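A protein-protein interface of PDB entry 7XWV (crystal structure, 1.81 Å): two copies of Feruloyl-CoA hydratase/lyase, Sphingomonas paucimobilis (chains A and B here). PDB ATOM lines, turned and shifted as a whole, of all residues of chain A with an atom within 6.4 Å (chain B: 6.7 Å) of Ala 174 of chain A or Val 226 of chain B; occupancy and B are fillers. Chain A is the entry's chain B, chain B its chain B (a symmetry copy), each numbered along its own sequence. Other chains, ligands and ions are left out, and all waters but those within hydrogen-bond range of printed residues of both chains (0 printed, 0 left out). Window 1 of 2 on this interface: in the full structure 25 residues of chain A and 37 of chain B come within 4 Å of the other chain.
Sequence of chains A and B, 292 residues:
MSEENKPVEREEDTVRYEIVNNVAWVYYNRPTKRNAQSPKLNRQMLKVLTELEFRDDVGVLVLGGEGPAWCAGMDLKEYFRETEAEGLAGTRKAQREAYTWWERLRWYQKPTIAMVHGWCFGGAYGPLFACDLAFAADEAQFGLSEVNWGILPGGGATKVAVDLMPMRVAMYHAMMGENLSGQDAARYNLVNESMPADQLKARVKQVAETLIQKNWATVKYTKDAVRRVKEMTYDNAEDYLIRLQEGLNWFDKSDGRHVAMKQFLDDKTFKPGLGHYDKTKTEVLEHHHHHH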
ATOM      1  N   LEU A 144       5.398   8.348  21.991  1.00  0.00           N
ATOM      2  CA  LEU A 144       5.652   9.493  22.895  1.00  0.00           C
ATOM      3  C   LEU A 144       4.896  10.672  22.279  1.00  0.00           C
ATOM      4  O   LEU A 144       5.494  11.423  21.437  1.00  0.00           O
ATOM      5  CB  LEU A 144       7.154   9.776  22.985  1.00  0.00           C
ATOM      6  CG  LEU A 144       8.040   8.654  23.511  1.00  0.00           C
ATOM      7  CD1 LEU A 144       9.496   9.057  23.458  1.00  0.00           C
ATOM      8  CD2 LEU A 144       7.667   8.211  24.938  1.00  0.00           C
ATOM      9  N   GLU A 146       3.791  13.154  23.870  1.00  0.00           N
ATOM     10  CA  GLU A 146       4.162  14.360  24.673  1.00  0.00           C
ATOM     11  C   GLU A 146       4.382  15.585  23.778  1.00  0.00           C
ATOM     12  O   GLU A 146       3.771  16.644  24.082  1.00  0.00           O
ATOM     13  CB  GLU A 146       5.402  14.112  25.540  1.00  0.00           C
ATOM     14  CG  GLU A 146       5.073  13.365  26.819  1.00  0.00           C
ATOM     15  CD  GLU A 146       5.197  11.854  26.734  1.00  0.00           C
ATOM     16  OE1 GLU A 146       5.684  11.272  27.722  1.00  0.00           O
ATOM     17  OE2 GLU A 146       4.851  11.264  25.663  1.00  0.00           O
ATOM     18  N   VAL A 147       5.217  15.479  22.743  1.00  0.00           N
ATOM     19  CA  VAL A 147       5.582  16.638  21.880  1.00  0.00           C
ATOM     20  C   VAL A 147       4.305  17.262  21.290  1.00  0.00           C
ATOM     21  O   VAL A 147       4.317  18.448  21.042  1.00  0.00           O
ATOM     22  CB  VAL A 147       6.598  16.239  20.794  1.00  0.00           C
ATOM     23  CG1 VAL A 147       6.027  15.259  19.786  1.00  0.00           C
ATOM     24  CG2 VAL A 147       7.173  17.434  20.078  1.00  0.00           C
ATOM     25  N   PRO A 153       9.090  14.520  26.602  1.00  0.00           N
ATOM     26  CA  PRO A 153       8.803  13.173  27.113  1.00  0.00           C
ATOM     27  C   PRO A 153       9.455  12.961  28.495  1.00  0.00           C
ATOM     28  O   PRO A 153      10.643  12.664  28.570  1.00  0.00           O
ATOM     29  CB  PRO A 153       9.338  12.253  26.004  1.00  0.00           C
ATOM     30  CG  PRO A 153       9.553  13.184  24.814  1.00  0.00           C
ATOM     31  CD  PRO A 153       9.949  14.502  25.421  1.00  0.00           C
ATOM     32  N   THR A 158      11.849   9.765  27.728  1.00  0.00           N
ATOM     33  CA  THR A 158      12.956  10.042  26.761  1.00  0.00           C
ATOM     34  C   THR A 158      14.172   9.115  26.972  1.00  0.00           C
ATOM     35  O   THR A 158      14.802   8.676  25.982  1.00  0.00           O
ATOM     36  CB  THR A 158      13.438  11.495  26.841  1.00  0.00           C
ATOM     37  OG1 THR A 158      12.365  12.369  26.490  1.00  0.00           O
ATOM     38  CG2 THR A 158      14.596  11.761  25.907  1.00  0.00           C
ATOM     39  N   ALA A 161      13.425   5.508  25.745  1.00  0.00           N
ATOM     40  CA  ALA A 161      13.536   5.484  24.265  1.00  0.00           C
ATOM     41  C   ALA A 161      14.995   5.322  23.850  1.00  0.00           C
ATOM     42  O   ALA A 161      15.289   4.444  23.062  1.00  0.00           O
ATOM     43  CB  ALA A 161      12.933   6.724  23.710  1.00  0.00           C
ATOM     44  N   VAL A 162      15.890   6.108  24.439  1.00  0.00           N
ATOM     45  CA  VAL A 162      17.348   6.121  24.110  1.00  0.00           C
ATOM     46  C   VAL A 162      18.033   4.843  24.616  1.00  0.00           C
ATOM     47  O   VAL A 162      19.006   4.398  23.987  1.00  0.00           O
ATOM     48  CB  VAL A 162      17.927   7.400  24.738  1.00  0.00           C
ATOM     49  CG1 VAL A 162      19.354   7.275  25.198  1.00  0.00           C
ATOM     50  CG2 VAL A 162      17.729   8.551  23.776  1.00  0.00           C
ATOM     51  N   MET A 167      19.605   5.382  18.485  1.00  0.00           N
ATOM     52  CA  MET A 167      19.485   6.838  18.745  1.00  0.00           C
ATOM     53  C   MET A 167      18.667   7.524  17.639  1.00  0.00           C
ATOM     54  O   MET A 167      17.769   8.290  18.002  1.00  0.00           O
ATOM     55  CB  MET A 167      20.855   7.491  18.873  1.00  0.00           C
ATOM     56  CG  MET A 167      20.777   8.982  19.113  1.00  0.00           C
ATOM     57  SD  MET A 167      22.373   9.745  18.737  1.00  0.00           S
ATOM     58  CE  MET A 167      22.093  11.475  19.131  1.00  0.00           C
ATOM     59  N   VAL A 169      16.276   6.285  15.909  1.00  0.00           N
ATOM     60  CA  VAL A 169      14.871   5.849  16.108  1.00  0.00           C
ATOM     61  C   VAL A 169      14.294   6.557  17.331  1.00  0.00           C
ATOM     62  O   VAL A 169      13.150   7.059  17.216  1.00  0.00           O
ATOM     63  CB  VAL A 169      14.744   4.318  16.164  1.00  0.00           C
ATOM     64  CG1 VAL A 169      13.310   3.909  16.453  1.00  0.00           C
ATOM     65  CG2 VAL A 169      15.236   3.746  14.841  1.00  0.00           C
ATOM     66  N   ALA A 170      15.057   6.689  18.419  1.00  0.00           N
ATOM     67  CA  ALA A 170      14.575   7.381  19.633  1.00  0.00           C
ATOM     68  C   ALA A 170      14.296   8.830  19.241  1.00  0.00           C
ATOM     69  O   ALA A 170      13.269   9.381  19.661  1.00  0.00           O
ATOM     70  CB  ALA A 170      15.584   7.324  20.755  1.00  0.00           C
ATOM     71  N   MET A 171      15.169   9.408  18.424  1.00  0.00           N
ATOM     72  CA  MET A 171      15.094  10.841  18.082  1.00  0.00           C
ATOM     73  C   MET A 171      13.798  11.072  17.311  1.00  0.00           C
ATOM     74  O   MET A 171      13.052  11.975  17.665  1.00  0.00           O
ATOM     75  CB  MET A 171      16.309  11.289  17.257  1.00  0.00           C
ATOM     76  CG  MET A 171      16.310  12.728  16.935  1.00  0.00           C
ATOM     77  SD  MET A 171      16.529  13.779  18.404  1.00  0.00           S
ATOM     78  CE  MET A 171      18.235  13.473  18.812  1.00  0.00           C
ATOM     79  N   TYR A 172      13.539  10.273  16.291  1.00  0.00           N
ATOM     80  CA  TYR A 172      12.308  10.361  15.490  1.00  0.00           C
ATOM     81  C   TYR A 172      11.064  10.145  16.370  1.00  0.00           C
ATOM     82  O   TYR A 172      10.107  10.930  16.287  1.00  0.00           O
ATOM     83  CB  TYR A 172      12.351   9.356  14.345  1.00  0.00           C
ATOM     84  CG  TYR A 172      11.222   9.530  13.356  1.00  0.00           C
ATOM     85  CD1 TYR A 172       9.949   9.007  13.602  1.00  0.00           C
ATOM     86  CD2 TYR A 172      11.424  10.204  12.165  1.00  0.00           C
ATOM     87  CE1 TYR A 172       8.913   9.183  12.680  1.00  0.00           C
ATOM     88  CE2 TYR A 172      10.410  10.377  11.235  1.00  0.00           C
ATOM     89  CZ  TYR A 172       9.154   9.858  11.484  1.00  0.00           C
ATOM     90  OH  TYR A 172       8.179  10.032  10.525  1.00  0.00           O
ATOM     91  N   HIS A 173      11.079   9.095  17.179  1.00  0.00           N
ATOM     92  CA  HIS A 173       9.973   8.701  18.097  1.00  0.00           C
ATOM     93  C   HIS A 173       9.599   9.887  18.997  1.00  0.00           C
ATOM     94  O   HIS A 173       8.415  10.199  19.130  1.00  0.00           O
ATOM     95  CB  HIS A 173      10.409   7.491  18.911  1.00  0.00           C
ATOM     96  CG  HIS A 173       9.238   6.740  19.421  1.00  0.00           C
ATOM     97  ND1 HIS A 173       9.003   6.554  20.773  1.00  0.00           N
ATOM     98  CD2 HIS A 173       8.242   6.133  18.754  1.00  0.00           C
ATOM     99  CE1 HIS A 173       7.891   5.859  20.924  1.00  0.00           C
ATOM    100  NE2 HIS A 173       7.387   5.605  19.701  1.00  0.00           N
ATOM    101  N   ALA A 174      10.595  10.531  19.607  1.00  0.00           N
ATOM    102  CA  ALA A 174      10.402  11.641  20.556  1.00  0.00           C
ATOM    103  C   ALA A 174       9.987  12.935  19.838  1.00  0.00           C
ATOM    104  O   ALA A 174       9.107  13.621  20.392  1.00  0.00           O
ATOM    105  CB  ALA A 174      11.640  11.832  21.368  1.00  0.00           C
ATOM    106  N   MET A 175      10.592  13.253  18.685  1.00  0.00           N
ATOM    107  CA  MET A 175      10.400  14.552  17.985  1.00  0.00           C
ATOM    108  C   MET A 175       9.116  14.561  17.163  1.00  0.00           C
ATOM    109  O   MET A 175       8.461  15.652  17.115  1.00  0.00           O
ATOM    110  CB  MET A 175      11.553  14.823  17.026  1.00  0.00           C
ATOM    111  CG  MET A 175      12.872  15.125  17.696  1.00  0.00           C
ATOM    112  SD  MET A 175      14.116  15.436  16.398  1.00  0.00           S
ATOM    113  CE  MET A 175      13.685  17.122  15.988  1.00  0.00           C
ATOM    114  N   MET A 176       8.739  13.428  16.559  1.00  0.00           N
ATOM    115  CA  MET A 176       7.587  13.390  15.618  1.00  0.00           C
ATOM    116  C   MET A 176       6.301  12.985  16.336  1.00  0.00           C
ATOM    117  O   MET A 176       5.255  13.282  15.790  1.00  0.00           O
ATOM    118  CB  MET A 176       7.871  12.471  14.434  1.00  0.00           C
ATOM    119  CG  MET A 176       9.104  12.889  13.682  1.00  0.00           C
ATOM    120  SD  MET A 176       8.812  14.415  12.755  1.00  0.00           S
ATOM    121  CE  MET A 176       7.821  13.779  11.412  1.00  0.00           C
ATOM    122  N   GLY A 177       6.387  12.355  17.518  1.00  0.00           N
ATOM    123  CA  GLY A 177       5.229  11.863  18.281  1.00  0.00           C
ATOM    124  C   GLY A 177       4.336  10.933  17.467  1.00  0.00           C
ATOM    125  O   GLY A 177       3.119  10.936  17.717  1.00  0.00           O
ATOM    126  N   LYS B 214       4.488  21.759  15.136  1.00  0.00           N
ATOM    127  CA  LYS B 214       4.646  21.497  16.598  1.00  0.00           C
ATOM    128  C   LYS B 214       5.073  22.799  17.287  1.00  0.00           C
ATOM    129  O   LYS B 214       5.462  23.709  16.609  1.00  0.00           O
ATOM    130  CB  LYS B 214       5.601  20.319  16.823  1.00  0.00           C
ATOM    131  CG  LYS B 214       5.132  19.048  16.116  1.00  0.00           C
ATOM    132  CD  LYS B 214       5.931  17.786  16.371  1.00  0.00           C
ATOM    133  CE  LYS B 214       5.500  16.642  15.467  1.00  0.00           C
ATOM    134  NZ  LYS B 214       4.091  16.229  15.700  1.00  0.00           N
ATOM    135  N   TYR B 221      13.697  21.453  23.107  1.00  0.00           N
ATOM    136  CA  TYR B 221      13.967  20.814  24.423  1.00  0.00           C
ATOM    137  C   TYR B 221      13.966  19.281  24.283  1.00  0.00           C
ATOM    138  O   TYR B 221      14.749  18.626  24.910  1.00  0.00           O
ATOM    139  CB  TYR B 221      12.954  21.282  25.456  1.00  0.00           C
ATOM    140  CG  TYR B 221      13.379  22.516  26.176  1.00  0.00           C
ATOM    141  CD1 TYR B 221      13.033  23.770  25.709  1.00  0.00           C
ATOM    142  CD2 TYR B 221      14.091  22.420  27.352  1.00  0.00           C
ATOM    143  CE1 TYR B 221      13.401  24.916  26.401  1.00  0.00           C
ATOM    144  CE2 TYR B 221      14.498  23.554  28.027  1.00  0.00           C
ATOM    145  CZ  TYR B 221      14.127  24.799  27.564  1.00  0.00           C
ATOM    146  OH  TYR B 221      14.533  25.912  28.233  1.00  0.00           O
ATOM    147  N   THR B 222      13.080  18.715  23.472  1.00  0.00           N
ATOM    148  CA  THR B 222      13.027  17.269  23.207  1.00  0.00           C
ATOM    149  C   THR B 222      14.304  16.779  22.492  1.00  0.00           C
ATOM    150  O   THR B 222      14.863  15.787  22.987  1.00  0.00           O
ATOM    151  CB  THR B 222      11.750  16.887  22.456  1.00  0.00           C
ATOM    152  OG1 THR B 222      10.638  17.184  23.304  1.00  0.00           O
ATOM    153  CG2 THR B 222      11.732  15.427  22.092  1.00  0.00           C
ATOM    154  N   LYS B 223      14.718  17.369  21.355  1.00  0.00           N
ATOM    155  CA  LYS B 223      15.886  16.846  20.613  1.00  0.00           C
ATOM    156  C   LYS B 223      17.132  17.004  21.477  1.00  0.00           C
ATOM    157  O   LYS B 223      17.967  16.116  21.433  1.00  0.00           O
ATOM    158  CB  LYS B 223      16.072  17.520  19.253  1.00  0.00           C
ATOM    159  CG  LYS B 223      16.623  18.925  19.277  1.00  0.00           C
ATOM    160  CD  LYS B 223      16.088  19.714  18.082  1.00  0.00           C
ATOM    161  CE  LYS B 223      16.959  20.893  17.721  1.00  0.00           C
ATOM    162  NZ  LYS B 223      18.324  20.474  17.306  1.00  0.00           N
ATOM    163  N   ASP B 224      17.275  18.101  22.217  1.00  0.00           N
ATOM    164  CA  ASP B 224      18.420  18.216  23.144  1.00  0.00           C
ATOM    165  C   ASP B 224      18.354  17.126  24.216  1.00  0.00           C
ATOM    166  O   ASP B 224      19.437  16.561  24.512  1.00  0.00           O
ATOM    167  CB  ASP B 224      18.492  19.585  23.829  1.00  0.00           C
ATOM    168  CG  ASP B 224      19.165  20.636  22.972  1.00  0.00           C
ATOM    169  OD1 ASP B 224      19.275  20.403  21.736  1.00  0.00           O
ATOM    170  OD2 ASP B 224      19.630  21.665  23.565  1.00  0.00           O
ATOM    171  N   ALA B 225      17.191  16.875  24.822  1.00  0.00           N
ATOM    172  CA  ALA B 225      17.035  15.804  25.836  1.00  0.00           C
ATOM    173  C   ALA B 225      17.529  14.463  25.284  1.00  0.00           C
ATOM    174  O   ALA B 225      18.284  13.768  25.962  1.00  0.00           O
ATOM    175  CB  ALA B 225      15.611  15.698  26.327  1.00  0.00           C
ATOM    176  N   VAL B 226      17.067  14.066  24.116  1.00  0.00           N
ATOM    177  CA  VAL B 226      17.466  12.780  23.501  1.00  0.00           C
ATOM    178  C   VAL B 226      18.980  12.717  23.437  1.00  0.00           C
ATOM    179  O   VAL B 226      19.567  11.715  23.937  1.00  0.00           O
ATOM    180  CB  VAL B 226      16.813  12.603  22.127  1.00  0.00           C
ATOM    181  CG1 VAL B 226      17.405  11.424  21.387  1.00  0.00           C
ATOM    182  CG2 VAL B 226      15.316  12.436  22.281  1.00  0.00           C
ATOM    183  N   ARG B 227      19.606  13.769  22.942  1.00  0.00           N
ATOM    184  CA  ARG B 227      21.077  13.758  22.788  1.00  0.00           C
ATOM    185  C   ARG B 227      21.738  13.703  24.170  1.00  0.00           C
ATOM    186  O   ARG B 227      22.784  13.010  24.316  1.00  0.00           O
ATOM    187  CB  ARG B 227      21.572  14.996  22.034  1.00  0.00           C
ATOM    188  CG  ARG B 227      21.161  15.088  20.584  1.00  0.00           C
ATOM    189  CD  ARG B 227      21.884  16.263  19.898  1.00  0.00           C
ATOM    190  NE  ARG B 227      21.611  16.336  18.477  1.00  0.00           N
ATOM    191  CZ  ARG B 227      22.201  15.590  17.553  1.00  0.00           C
ATOM    192  NH1 ARG B 227      23.116  14.694  17.889  1.00  0.00           N
ATOM    193  NH2 ARG B 227      21.858  15.729  16.287  1.00  0.00           N
ATOM    194  N   ARG B 228      21.195  14.394  25.150  1.00  0.00           N
ATOM    195  CA  ARG B 228      21.911  14.542  26.450  1.00  0.00           C
ATOM    196  C   ARG B 228      21.728  13.277  27.310  1.00  0.00           C
ATOM    197  O   ARG B 228      22.589  12.987  28.085  1.00  0.00           O
ATOM    198  CB  ARG B 228      21.369  15.754  27.210  1.00  0.00           C
ATOM    199  CG  ARG B 228      21.719  17.074  26.530  1.00  0.00           C
ATOM    200  CD  ARG B 228      23.066  17.589  26.984  1.00  0.00           C
ATOM    201  NE  ARG B 228      23.415  18.825  26.297  1.00  0.00           N
ATOM    202  CZ  ARG B 228      24.639  19.335  26.230  1.00  0.00           C
ATOM    203  NH1 ARG B 228      25.647  18.744  26.847  1.00  0.00           N
ATOM    204  NH2 ARG B 228      24.851  20.468  25.577  1.00  0.00           N
ATOM    205  N   VAL B 229      20.585  12.595  27.258  1.00  0.00           N
ATOM    206  CA  VAL B 229      20.304  11.588  28.312  1.00  0.00           C
ATOM    207  C   VAL B 229      21.110  10.315  27.971  1.00  0.00           C
ATOM    208  O   VAL B 229      21.241   9.464  28.826  1.00  0.00           O
ATOM    209  CB  VAL B 229      18.812  11.358  28.532  1.00  0.00           C
ATOM    210  CG1 VAL B 229      18.150  12.613  29.059  1.00  0.00           C
ATOM    211  CG2 VAL B 229      18.125  10.833  27.289  1.00  0.00           C
ATOM    212  N   LYS B 230      21.674  10.250  26.774  1.00  0.00           N
ATOM    213  CA  LYS B 230      22.586   9.165  26.349  1.00  0.00           C
ATOM    214  C   LYS B 230      23.858   9.128  27.193  1.00  0.00           C
ATOM    215  O   LYS B 230      24.357   8.022  27.362  1.00  0.00           O
ATOM    216  CB  LYS B 230      22.946   9.272  24.871  1.00  0.00           C
ATOM    217  CG  LYS B 230      23.391   7.934  24.292  1.00  0.00           C
ATOM    218  CD  LYS B 230      23.140   7.866  22.803  1.00  0.00           C
ATOM    219  CE  LYS B 230      23.504   6.543  22.160  1.00  0.00           C
ATOM    220  NZ  LYS B 230      23.789   6.739  20.724  1.00  0.00           N
ATOM    221  N   GLU B 231      24.295  10.252  27.765  1.00  0.00           N
ATOM    222  CA  GLU B 231      25.567  10.385  28.544  1.00  0.00           C
ATOM    223  C   GLU B 231      25.241  10.547  30.034  1.00  0.00           C
ATOM    224  O   GLU B 231      26.027  11.205  30.781  1.00  0.00           O
ATOM    225  CB  GLU B 231      26.390  11.531  27.957  1.00  0.00           C
ATOM    226  CG  GLU B 231      26.889  11.202  26.559  1.00  0.00           C
ATOM    227  CD  GLU B 231      27.747  12.263  25.883  1.00  0.00           C
ATOM    228  OE1 GLU B 231      27.872  13.390  26.476  1.00  0.00           O
ATOM    229  OE2 GLU B 231      28.279  11.961  24.766  1.00  0.00           O
ATOM    230  N   LEU B 241      15.221  15.442  33.235  1.00  0.00           N
ATOM    231  CA  LEU B 241      14.052  15.712  32.375  1.00  0.00           C
ATOM    232  C   LEU B 241      13.041  16.590  33.120  1.00  0.00           C
ATOM    233  O   LEU B 241      12.441  17.416  32.509  1.00  0.00           O
ATOM    234  CB  LEU B 241      13.467  14.383  31.892  1.00  0.00           C
ATOM    235  CG  LEU B 241      14.366  13.602  30.944  1.00  0.00           C
ATOM    236  CD1 LEU B 241      13.980  12.127  30.894  1.00  0.00           C
ATOM    237  CD2 LEU B 241      14.328  14.201  29.550  1.00  0.00           C
ATOM    238  N   LEU B 244      14.459  19.992  32.879  1.00  0.00           N
ATOM    239  CA  LEU B 244      14.288  20.523  31.515  1.00  0.00           C
ATOM    240  C   LEU B 244      12.882  21.127  31.352  1.00  0.00           C
ATOM    241  O   LEU B 244      12.791  22.199  30.744  1.00  0.00           O
ATOM    242  CB  LEU B 244      14.554  19.430  30.481  1.00  0.00           C
ATOM    243  CG  LEU B 244      16.021  19.049  30.234  1.00  0.00           C
ATOM    244  CD1 LEU B 244      16.108  18.165  29.003  1.00  0.00           C
ATOM    245  CD2 LEU B 244      16.936  20.258  30.076  1.00  0.00           C
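The backbone carbonyl oxygen (O) of Met 176 of chain A sits at hydrogen-bond distance from the side-chain amino group (NZ) of Lys 214 of chain B.
The backbone carbonyl oxygen of Pro 153 of chain A sits at hydrogen-bond distance from the side-chain hydroxyl of Thr 158 of chain A, at 2.7 Å.
Lys 214 of chain B touches Val 147 of chain A (CD to CG2, 3.9 Å). Thr 158 of chain A touches Leu 241 of chain B (CB to CD2, 3.9 Å). CG2 of Val 162 of chain A touches O of Val 226 of chain B, at 3.7 Å. CG1 of Val 162 of chain A touches CA of Lys 230 of chain B, at 3.9 Å. CE of Met 167 of chain A touches NH1 of Arg 227 of chain B, at 3.6 Å. Lys 230 of chain B touches Met 167 of chain A. CE of Met 171 of chain A touches O of Lys 223 of chain B (3.7 Å). CG1 of Val 226 of chain B touches CE of Met 171 of chain A (3.4 Å). Met 171 of chain A touches Arg 227 of chain B (CE to CG, 3.8 Å). CB of Ala 174 of chain A touches CG2 of Val 226 of chain B (3.8 Å).
Of chain B, only Thr 222 and Val 226 come within 4 Å of Ala 174 of chain A. Val 226 of chain B touches just these residues of chain A: Thr 158 (3.8 Å), Val 162 (3.7 Å), Met 171 (3.4 Å) and Ala 174 (3.8 Å). Of the printed residues of chain A, Val 229 of chain B touches Thr 158. Of the printed residues of chain B, Met 175 of chain A touches Lys 214. Leu 244 of chain B touches none of the printed residues of chain A. Ala 161 of chain A touches none of the printed residues of chain B.
Hydrophobic or aromatic side chains of chain A that line the printed part of chain B: Val 147, Pro 153, Val 162, Met 167, Met 171 and Ala 174. Hydrophobic or aromatic side chains of chain B within 4 Å of the printed part of chain A: Val 226, Val 229 and Leu 241.
No position is printed for both chains. Of the 16 pairs that touch across the chains among the printed residues, none has its exchanged pair printed and touching as well.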
